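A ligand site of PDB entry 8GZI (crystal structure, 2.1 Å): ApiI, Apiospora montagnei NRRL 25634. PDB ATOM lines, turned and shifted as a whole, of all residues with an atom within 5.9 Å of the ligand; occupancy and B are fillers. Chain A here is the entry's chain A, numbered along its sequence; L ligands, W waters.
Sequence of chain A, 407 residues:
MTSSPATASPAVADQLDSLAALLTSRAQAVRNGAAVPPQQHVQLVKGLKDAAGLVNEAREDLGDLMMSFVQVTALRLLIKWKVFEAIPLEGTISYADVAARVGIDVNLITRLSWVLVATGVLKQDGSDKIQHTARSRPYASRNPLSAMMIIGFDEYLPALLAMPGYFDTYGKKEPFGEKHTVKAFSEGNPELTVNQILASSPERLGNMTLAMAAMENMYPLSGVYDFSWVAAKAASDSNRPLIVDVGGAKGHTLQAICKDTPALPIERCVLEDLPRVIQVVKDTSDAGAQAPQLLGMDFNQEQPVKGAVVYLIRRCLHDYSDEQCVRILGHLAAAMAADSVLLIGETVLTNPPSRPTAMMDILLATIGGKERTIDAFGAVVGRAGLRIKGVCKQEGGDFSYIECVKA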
ATOM      1  N   GLU A 216     -23.481  -5.146  -6.136  1.00  0.00           N
ATOM      2  CA  GLU A 216     -22.182  -4.539  -5.865  1.00  0.00           C
ATOM      3  C   GLU A 216     -21.129  -5.617  -5.628  1.00  0.00           C
ATOM      4  O   GLU A 216     -19.950  -5.421  -5.950  1.00  0.00           O
ATOM      5  CB  GLU A 216     -22.266  -3.605  -4.659  1.00  0.00           C
ATOM      6  CG  GLU A 216     -21.070  -2.674  -4.495  1.00  0.00           C
ATOM      7  CD  GLU A 216     -21.027  -1.585  -5.539  1.00  0.00           C
ATOM      8  OE1 GLU A 216     -22.095  -1.166  -6.024  1.00  0.00           O
ATOM      9  OE2 GLU A 216     -19.909  -1.144  -5.886  1.00  0.00           O
ATOM     10  N   ASP A 245      -6.780  -0.870 -10.365  1.00  0.00           N
ATOM     11  CA  ASP A 245      -8.207  -1.125 -10.609  1.00  0.00           C
ATOM     12  C   ASP A 245      -8.729  -0.016 -11.509  1.00  0.00           C
ATOM     13  O   ASP A 245      -9.020   1.091 -11.061  1.00  0.00           O
ATOM     14  CB  ASP A 245      -8.979  -1.212  -9.290  1.00  0.00           C
ATOM     15  CG  ASP A 245     -10.418  -1.720  -9.470  1.00  0.00           C
ATOM     16  OD1 ASP A 245     -10.820  -2.074 -10.603  1.00  0.00           O
ATOM     17  OD2 ASP A 245     -11.143  -1.784  -8.458  1.00  0.00           O
ATOM     18  N   VAL A 246      -8.810  -0.301 -12.809  1.00  0.00           N
ATOM     19  CA  VAL A 246      -9.129   0.718 -13.807  1.00  0.00           C
ATOM     20  C   VAL A 246     -10.635   0.922 -13.838  1.00  0.00           C
ATOM     21  O   VAL A 246     -11.394   0.015 -14.187  1.00  0.00           O
ATOM     22  CB  VAL A 246      -8.592   0.304 -15.188  1.00  0.00           C
ATOM     23  CG1 VAL A 246      -8.793   1.406 -16.203  1.00  0.00           C
ATOM     24  CG2 VAL A 246      -7.096  -0.067 -15.079  1.00  0.00           C
ATOM     25  N   GLY A 247     -11.069   2.124 -13.462  1.00  0.00           N
ATOM     26  CA  GLY A 247     -12.499   2.369 -13.310  1.00  0.00           C
ATOM     27  C   GLY A 247     -13.096   1.583 -12.169  1.00  0.00           C
ATOM     28  O   GLY A 247     -14.185   0.998 -12.325  1.00  0.00           O
ATOM     29  N   GLY A 248     -12.421   1.539 -11.030  1.00  0.00           N
ATOM     30  CA  GLY A 248     -12.815   0.715  -9.905  1.00  0.00           C
ATOM     31  C   GLY A 248     -13.801   1.338  -8.940  1.00  0.00           C
ATOM     32  O   GLY A 248     -13.991   0.787  -7.847  1.00  0.00           O
ATOM     33  N   ALA A 249     -14.426   2.456  -9.298  1.00  0.00           N
ATOM     34  CA  ALA A 249     -15.477   3.087  -8.498  1.00  0.00           C
ATOM     35  C   ALA A 249     -14.979   3.433  -7.107  1.00  0.00           C
ATOM     36  O   ALA A 249     -14.192   4.362  -6.932  1.00  0.00           O
ATOM     37  CB  ALA A 249     -16.722   2.195  -8.407  1.00  0.00           C
ATOM     38  N   LYS A 250     -15.455   2.719  -6.096  1.00  0.00           N
ATOM     39  CA  LYS A 250     -15.066   3.024  -4.735  1.00  0.00           C
ATOM     40  C   LYS A 250     -13.995   2.088  -4.199  1.00  0.00           C
ATOM     41  O   LYS A 250     -13.616   2.196  -3.036  1.00  0.00           O
ATOM     42  CB  LYS A 250     -16.309   3.048  -3.840  1.00  0.00           C
ATOM     43  CG  LYS A 250     -17.405   3.992  -4.390  1.00  0.00           C
ATOM     44  CD  LYS A 250     -18.811   3.664  -3.888  1.00  0.00           C
ATOM     45  CE  LYS A 250     -19.583   4.928  -3.495  1.00  0.00           C
ATOM     46  NZ  LYS A 250     -19.683   5.942  -4.596  1.00  0.00           N
ATOM     47  N   THR A 253     -13.441  -3.797  -4.715  1.00  0.00           N
ATOM     48  CA  THR A 253     -12.745  -4.973  -5.231  1.00  0.00           C
ATOM     49  C   THR A 253     -11.290  -5.019  -4.765  1.00  0.00           C
ATOM     50  O   THR A 253     -10.772  -6.080  -4.423  1.00  0.00           O
ATOM     51  CB  THR A 253     -12.805  -4.982  -6.762  1.00  0.00           C
ATOM     52  OG1 THR A 253     -14.156  -4.780  -7.182  1.00  0.00           O
ATOM     53  CG2 THR A 253     -12.310  -6.314  -7.300  1.00  0.00           C
ATOM     54  N   GLU A 272      -8.293   3.807  -9.802  1.00  0.00           N
ATOM     55  CA  GLU A 272      -8.464   4.828 -10.834  1.00  0.00           C
ATOM     56  C   GLU A 272      -9.931   4.956 -11.199  1.00  0.00           C
ATOM     57  O   GLU A 272     -10.630   3.950 -11.344  1.00  0.00           O
ATOM     58  CB  GLU A 272      -7.676   4.475 -12.113  1.00  0.00           C
ATOM     59  CG  GLU A 272      -6.195   4.384 -11.902  1.00  0.00           C
ATOM     60  CD  GLU A 272      -5.444   3.978 -13.154  1.00  0.00           C
ATOM     61  OE1 GLU A 272      -6.064   3.440 -14.101  1.00  0.00           O
ATOM     62  OE2 GLU A 272      -4.221   4.213 -13.199  1.00  0.00           O
ATOM     63  N   ASP A 273     -10.383   6.194 -11.362  1.00  0.00           N
ATOM     64  CA  ASP A 273     -11.723   6.500 -11.837  1.00  0.00           C
ATOM     65  C   ASP A 273     -11.716   7.972 -12.206  1.00  0.00           C
ATOM     66  O   ASP A 273     -10.695   8.661 -12.058  1.00  0.00           O
ATOM     67  CB  ASP A 273     -12.794   6.145 -10.805  1.00  0.00           C
ATOM     68  CG  ASP A 273     -14.073   5.633 -11.449  1.00  0.00           C
ATOM     69  OD1 ASP A 273     -14.753   6.428 -12.109  1.00  0.00           O
ATOM     70  OD2 ASP A 273     -14.392   4.427 -11.326  1.00  0.00           O
ATOM     71  N   LEU A 274     -12.845   8.452 -12.700  1.00  0.00           N
ATOM     72  CA  LEU A 274     -12.969   9.872 -13.033  1.00  0.00           C
ATOM     73  C   LEU A 274     -12.678  10.728 -11.796  1.00  0.00           C
ATOM     74  O   LEU A 274     -12.906  10.309 -10.660  1.00  0.00           O
ATOM     75  CB  LEU A 274     -14.373  10.182 -13.546  1.00  0.00           C
ATOM     76  CG  LEU A 274     -14.837   9.356 -14.740  1.00  0.00           C
ATOM     77  CD1 LEU A 274     -16.346   9.465 -14.881  1.00  0.00           C
ATOM     78  CD2 LEU A 274     -14.127   9.818 -15.993  1.00  0.00           C
ATOM     79  N   VAL A 277     -15.506  11.013  -9.101  1.00  0.00           N
ATOM     80  CA  VAL A 277     -15.792   9.890  -8.205  1.00  0.00           C
ATOM     81  C   VAL A 277     -14.638   9.669  -7.235  1.00  0.00           C
ATOM     82  O   VAL A 277     -14.849   9.313  -6.067  1.00  0.00           O
ATOM     83  CB  VAL A 277     -16.118   8.629  -9.034  1.00  0.00           C
ATOM     84  CG1 VAL A 277     -15.129   8.500 -10.090  1.00  0.00           C
ATOM     85  CG2 VAL A 277     -16.090   7.374  -8.177  1.00  0.00           C
ATOM     86  N   MET A 297      -8.640   9.985 -13.443  1.00  0.00           N
ATOM     87  CA  MET A 297      -8.139   9.830 -14.812  1.00  0.00           C
ATOM     88  C   MET A 297      -9.302   9.471 -15.719  1.00  0.00           C
ATOM     89  O   MET A 297     -10.428   9.282 -15.274  1.00  0.00           O
ATOM     90  CB  MET A 297      -7.023   8.766 -14.896  1.00  0.00           C
ATOM     91  CG  MET A 297      -7.376   7.421 -14.268  1.00  0.00           C
ATOM     92  SD  MET A 297      -8.415   6.326 -15.276  1.00  0.00           S
ATOM     93  CE  MET A 297      -7.177   5.713 -16.437  1.00  0.00           C
ATOM     94  N   ASP A 298      -8.994   9.347 -17.009  1.00  0.00           N
ATOM     95  CA  ASP A 298      -9.973   8.978 -18.030  1.00  0.00           C
ATOM     96  C   ASP A 298      -9.389   7.797 -18.784  1.00  0.00           C
ATOM     97  O   ASP A 298      -8.369   7.938 -19.470  1.00  0.00           O
ATOM     98  CB  ASP A 298     -10.249  10.174 -18.945  1.00  0.00           C
ATOM     99  CG  ASP A 298     -11.213   9.858 -20.061  1.00  0.00           C
ATOM    100  OD1 ASP A 298     -11.676   8.699 -20.187  1.00  0.00           O
ATOM    101  OD2 ASP A 298     -11.505  10.782 -20.829  1.00  0.00           O
ATOM    102  N   PHE A 299     -10.017   6.623 -18.639  1.00  0.00           N
ATOM    103  CA  PHE A 299      -9.416   5.464 -19.288  1.00  0.00           C
ATOM    104  C   PHE A 299      -9.609   5.452 -20.804  1.00  0.00           C
ATOM    105  O   PHE A 299      -9.160   4.497 -21.454  1.00  0.00           O
ATOM    106  CB  PHE A 299      -9.886   4.143 -18.636  1.00  0.00           C
ATOM    107  CG  PHE A 299     -11.389   3.938 -18.549  1.00  0.00           C
ATOM    108  CD1 PHE A 299     -12.201   4.050 -19.671  1.00  0.00           C
ATOM    109  CD2 PHE A 299     -11.967   3.521 -17.354  1.00  0.00           C
ATOM    110  CE1 PHE A 299     -13.558   3.798 -19.580  1.00  0.00           C
ATOM    111  CE2 PHE A 299     -13.330   3.291 -17.254  1.00  0.00           C
ATOM    112  CZ  PHE A 299     -14.135   3.431 -18.364  1.00  0.00           C
ATOM    113  N   ASN A 300     -10.207   6.469 -21.402  1.00  0.00           N
ATOM    114  CA  ASN A 300     -10.140   6.615 -22.850  1.00  0.00           C
ATOM    115  C   ASN A 300      -8.867   7.311 -23.308  1.00  0.00           C
ATOM    116  O   ASN A 300      -8.628   7.407 -24.515  1.00  0.00           O
ATOM    117  CB  ASN A 300     -11.367   7.380 -23.363  1.00  0.00           C
ATOM    118  CG  ASN A 300     -12.680   6.663 -23.048  1.00  0.00           C
ATOM    119  OD1 ASN A 300     -12.976   5.606 -23.619  1.00  0.00           O
ATOM    120  ND2 ASN A 300     -13.445   7.231 -22.135  1.00  0.00           N
ATOM    121  N   ILE A 313      -9.908  -4.280 -15.122  1.00  0.00           N
ATOM    122  CA  ILE A 313     -11.004  -3.448 -15.642  1.00  0.00           C
ATOM    123  C   ILE A 313     -12.289  -4.273 -15.530  1.00  0.00           C
ATOM    124  O   ILE A 313     -12.534  -5.177 -16.335  1.00  0.00           O
ATOM    125  CB  ILE A 313     -10.747  -2.955 -17.086  1.00  0.00           C
ATOM    126  CG1 ILE A 313     -11.808  -1.953 -17.514  1.00  0.00           C
ATOM    127  CG2 ILE A 313     -10.544  -4.099 -18.101  1.00  0.00           C
ATOM    128  CD1 ILE A 313     -11.338  -1.006 -18.605  1.00  0.00           C
ATOM    129  N   ARG A 314     -13.084  -3.975 -14.510  1.00  0.00           N
ATOM    130  CA  ARG A 314     -14.206  -4.798 -14.102  1.00  0.00           C
ATOM    131  C   ARG A 314     -15.491  -4.066 -14.432  1.00  0.00           C
ATOM    132  O   ARG A 314     -15.672  -2.919 -14.014  1.00  0.00           O
ATOM    133  CB  ARG A 314     -14.109  -5.104 -12.598  1.00  0.00           C
ATOM    134  CG  ARG A 314     -15.058  -6.179 -12.114  1.00  0.00           C
ATOM    135  CD  ARG A 314     -15.108  -6.190 -10.590  1.00  0.00           C
ATOM    136  NE  ARG A 314     -15.762  -7.380 -10.078  1.00  0.00           N
ATOM    137  CZ  ARG A 314     -17.015  -7.410  -9.642  1.00  0.00           C
ATOM    138  NH1 ARG A 314     -17.753  -6.309  -9.671  1.00  0.00           N
ATOM    139  NH2 ARG A 314     -17.533  -8.534  -9.183  1.00  0.00           N
ATOM    140  N   ARG A 315     -16.347  -4.694 -15.240  1.00  0.00           N
ATOM    141  CA  ARG A 315     -17.676  -4.157 -15.525  1.00  0.00           C
ATOM    142  C   ARG A 315     -17.593  -2.747 -16.121  1.00  0.00           C
ATOM    143  O   ARG A 315     -18.408  -1.864 -15.819  1.00  0.00           O
ATOM    144  CB  ARG A 315     -18.555  -4.180 -14.260  1.00  0.00           C
ATOM    145  CG  ARG A 315     -18.931  -5.614 -13.834  1.00  0.00           C
ATOM    146  CD  ARG A 315     -19.885  -5.689 -12.618  1.00  0.00           C
ATOM    147  NE  ARG A 315     -20.831  -4.585 -12.607  1.00  0.00           N
ATOM    148  CZ  ARG A 315     -21.932  -4.525 -13.349  1.00  0.00           C
ATOM    149  NH1 ARG A 315     -22.257  -5.516 -14.179  1.00  0.00           N
ATOM    150  NH2 ARG A 315     -22.721  -3.445 -13.271  1.00  0.00           N
ATOM    151  N   CYS A 316     -16.603  -2.530 -16.984  1.00  0.00           N
ATOM    152  CA  CYS A 316     -16.541  -1.271 -17.730  1.00  0.00           C
ATOM    153  C   CYS A 316     -16.728  -1.439 -19.218  1.00  0.00           C
ATOM    154  O   CYS A 316     -17.470  -0.674 -19.835  1.00  0.00           O
ATOM    155  CB  CYS A 316     -15.200  -0.555 -17.487  1.00  0.00           C
ATOM    156  SG  CYS A 316     -14.944  -0.038 -15.761  1.00  0.00           S
ATOM    157  N   ASP A 319     -20.120  -1.258 -21.391  1.00  0.00           N
ATOM    158  CA  ASP A 319     -20.799   0.001 -21.664  1.00  0.00           C
ATOM    159  C   ASP A 319     -20.482   0.570 -23.046  1.00  0.00           C
ATOM    160  O   ASP A 319     -21.034   1.619 -23.391  1.00  0.00           O
ATOM    161  CB  ASP A 319     -20.408   1.035 -20.617  1.00  0.00           C
ATOM    162  CG  ASP A 319     -21.042   0.762 -19.248  1.00  0.00           C
ATOM    163  OD1 ASP A 319     -22.162   0.206 -19.221  1.00  0.00           O
ATOM    164  OD2 ASP A 319     -20.425   1.124 -18.232  1.00  0.00           O
ATOM    165  N   TYR A 320     -19.618  -0.067 -23.836  1.00  0.00           N
ATOM    166  CA  TYR A 320     -18.970   0.588 -24.979  1.00  0.00           C
ATOM    167  C   TYR A 320     -18.948  -0.300 -26.224  1.00  0.00           C
ATOM    168  O   TYR A 320     -19.013  -1.528 -26.156  1.00  0.00           O
ATOM    169  CB  TYR A 320     -17.536   0.980 -24.626  1.00  0.00           C
ATOM    170  CG  TYR A 320     -17.470   1.867 -23.403  1.00  0.00           C
ATOM    171  CD1 TYR A 320     -18.214   3.049 -23.348  1.00  0.00           C
ATOM    172  CD2 TYR A 320     -16.702   1.524 -22.318  1.00  0.00           C
ATOM    173  CE1 TYR A 320     -18.171   3.864 -22.237  1.00  0.00           C
ATOM    174  CE2 TYR A 320     -16.652   2.332 -21.187  1.00  0.00           C
ATOM    175  CZ  TYR A 320     -17.385   3.505 -21.158  1.00  0.00           C
ATOM    176  OH  TYR A 320     -17.334   4.326 -20.057  1.00  0.00           O
HETATM  177  N1  LIG L   1     -15.383  -1.626 -11.606  1.00  0.00           N
HETATM  178  C1  LIG L   1     -16.471  -1.224 -10.696  1.00  0.00           C
HETATM  179  C2  LIG L   1     -17.339  -0.121 -11.301  1.00  0.00           C
HETATM  180  C3  LIG L   1     -17.934  -0.410 -12.682  1.00  0.00           C
HETATM  181  S1  LIG L   1     -19.171   0.823 -13.193  1.00  0.00           S
HETATM  182  C4  LIG L   1     -17.364  -2.413 -10.328  1.00  0.00           C
HETATM  183  O1  LIG L   1     -16.941  -3.576 -10.372  1.00  0.00           O
HETATM  184  O2  LIG L   1     -18.526  -2.233  -9.990  1.00  0.00           O
HETATM  185  C5  LIG L   1     -18.088   1.692 -14.356  1.00  0.00           C
HETATM  186  C6  LIG L   1     -17.094   2.646 -13.698  1.00  0.00           C
HETATM  187  O3  LIG L   1     -16.309   3.265 -14.709  1.00  0.00           O
HETATM  188  C7  LIG L   1     -17.699   3.781 -12.870  1.00  0.00           C
HETATM  189  O4  LIG L   1     -17.040   3.834 -11.614  1.00  0.00           O
HETATM  190  C8  LIG L   1     -17.392   5.055 -13.646  1.00  0.00           C
HETATM  191  O5  LIG L   1     -17.037   6.128 -12.811  1.00  0.00           O
HETATM  192  C9  LIG L   1     -16.154   4.637 -14.419  1.00  0.00           C
HETATM  193  N2  LIG L   1     -15.913   5.378 -15.664  1.00  0.00           N
HETATM  194  C10 LIG L   1     -16.789   5.689 -16.683  1.00  0.00           C
HETATM  195  N3  LIG L   1     -16.107   6.368 -17.637  1.00  0.00           N
HETATM  196  C11 LIG L   1     -14.810   6.496 -17.245  1.00  0.00           C
HETATM  197  C12 LIG L   1     -13.694   7.086 -17.829  1.00  0.00           C
HETATM  198  N4  LIG L   1     -13.805   7.680 -19.008  1.00  0.00           N
HETATM  199  N5  LIG L   1     -12.476   7.058 -17.157  1.00  0.00           N
HETATM  200  C13 LIG L   1     -12.370   6.445 -15.924  1.00  0.00           C
HETATM  201  N6  LIG L   1     -13.486   5.854 -15.339  1.00  0.00           N
HETATM  202  C14 LIG L   1     -14.681   5.881 -16.004  1.00  0.00           C
HETATM  203  O   HOH W   1     -17.943   2.981 -17.859  1.00  0.00           O
HETATM  204  O   HOH W   2     -18.917   4.881  -9.694  1.00  0.00           O
HETATM  205  O   HOH W   3     -12.171  -1.897 -12.685  1.00  0.00           O
HETATM  206  O   HOH W   4     -13.532  -3.100  -9.549  1.00  0.00           O
HETATM  207  O   HOH W   5     -21.035  -1.710 -13.944  1.00  0.00           O
HETATM  208  O   HOH W   6     -16.161   6.854 -21.013  1.00  0.00           O
HETATM  209  O   HOH W   7     -17.758   8.229 -18.725  1.00  0.00           O
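The backbone carbonyl oxygen of Asp 273 is in hydrogen-bond range of the backbone NH of Met 297. The backbone NH (N) of Ala 249 sits at hydrogen-bond distance from the side-chain carboxylate (OD2) of Asp 273. N of Asn 300 lies within hydrogen-bond range of OD1 of Asp 298. The side-chain sulfur (SG) of Cys 316 is in hydrogen-bond range of the backbone carbonyl oxygen (O) of Arg 314 (3.4 Å). The backbone NH of Phe 299 sits close to the side-chain sulfur of Met 297 (3.7 Å). The backbone carbonyl oxygen (O) of Gly 247 lies within hydrogen-bond range of the side-chain sulfur (SG) of Cys 316 (3.7 Å). O of Glu 272 is in hydrogen-bond range of N of Gly 247, 2.8 Å away. O of Glu 272 is in hydrogen-bond range of N of Gly 248 (3.0 Å).
Residues that only touch the ligand: Gly 248, Ala 249, Leu 274, Met 297 and Arg 315. Within 4 Å of the ligand: Gly 247, Gly 248, Ala 249, Asp 273, Leu 274, Met 297, Asp 298, Phe 299, Asn 300, Arg 314, Arg 315, Cys 316 and Tyr 320.
O5 of the ligand is in hydrogen-bond range of OD1 of Asp 273, at 2.4 Å. OD1 of Asp 298 lies within hydrogen-bond range of N4 of the ligand (2.6 Å). A nitrogen (N1) of the ligand is in hydrogen-bond range of the backbone carbonyl oxygen (O) of Arg 314, at 2.7 Å. O1 of the ligand lies within salt-bridge range of NH1 of Arg 314. The backbone NH (N) of Phe 299 lies within hydrogen-bond range of a nitrogen (N5) of the ligand (2.9 Å). A nitrogen (N1) of the ligand is in hydrogen-bond range of the backbone carbonyl oxygen (O) of Gly 247 (3.0 Å). N4 of the ligand sits close to ND2 of Asn 300. N3 of the ligand lies within hydrogen-bond range of OH of Tyr 320, 3.4 Å away. An oxygen (O3) of the ligand lies within hydrogen-bond range of the side-chain sulfur of Cys 316, 3.7 Å away.
Water W4 lies within hydrogen-bond range of OD2 of Asp 245 (2.9 Å), OG1 of Thr 253 (3.0 Å) and N1 of the ligand (3.1 Å). Water W1 lies within hydrogen-bond range of OH of Tyr 320 (2.6 Å) and OD2 of Asp 319 (3.1 Å). Water W6 lies within hydrogen-bond range of OH of Tyr 320 (2.9 Å), ND2 of Asn 300 (3.0 Å) and N4 of the ligand (3.2 Å). Water W5 lies within hydrogen-bond range of NH2 of Arg 315 (2.5 Å) and S1 of the ligand (3.2 Å). Water W3 lies within hydrogen-bond range of the side-chain carboxylate of Asp 245, the backbone carbonyl oxygen of Val 246, the backbone NH of Arg 314 and a nitrogen (N1) of the ligand.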
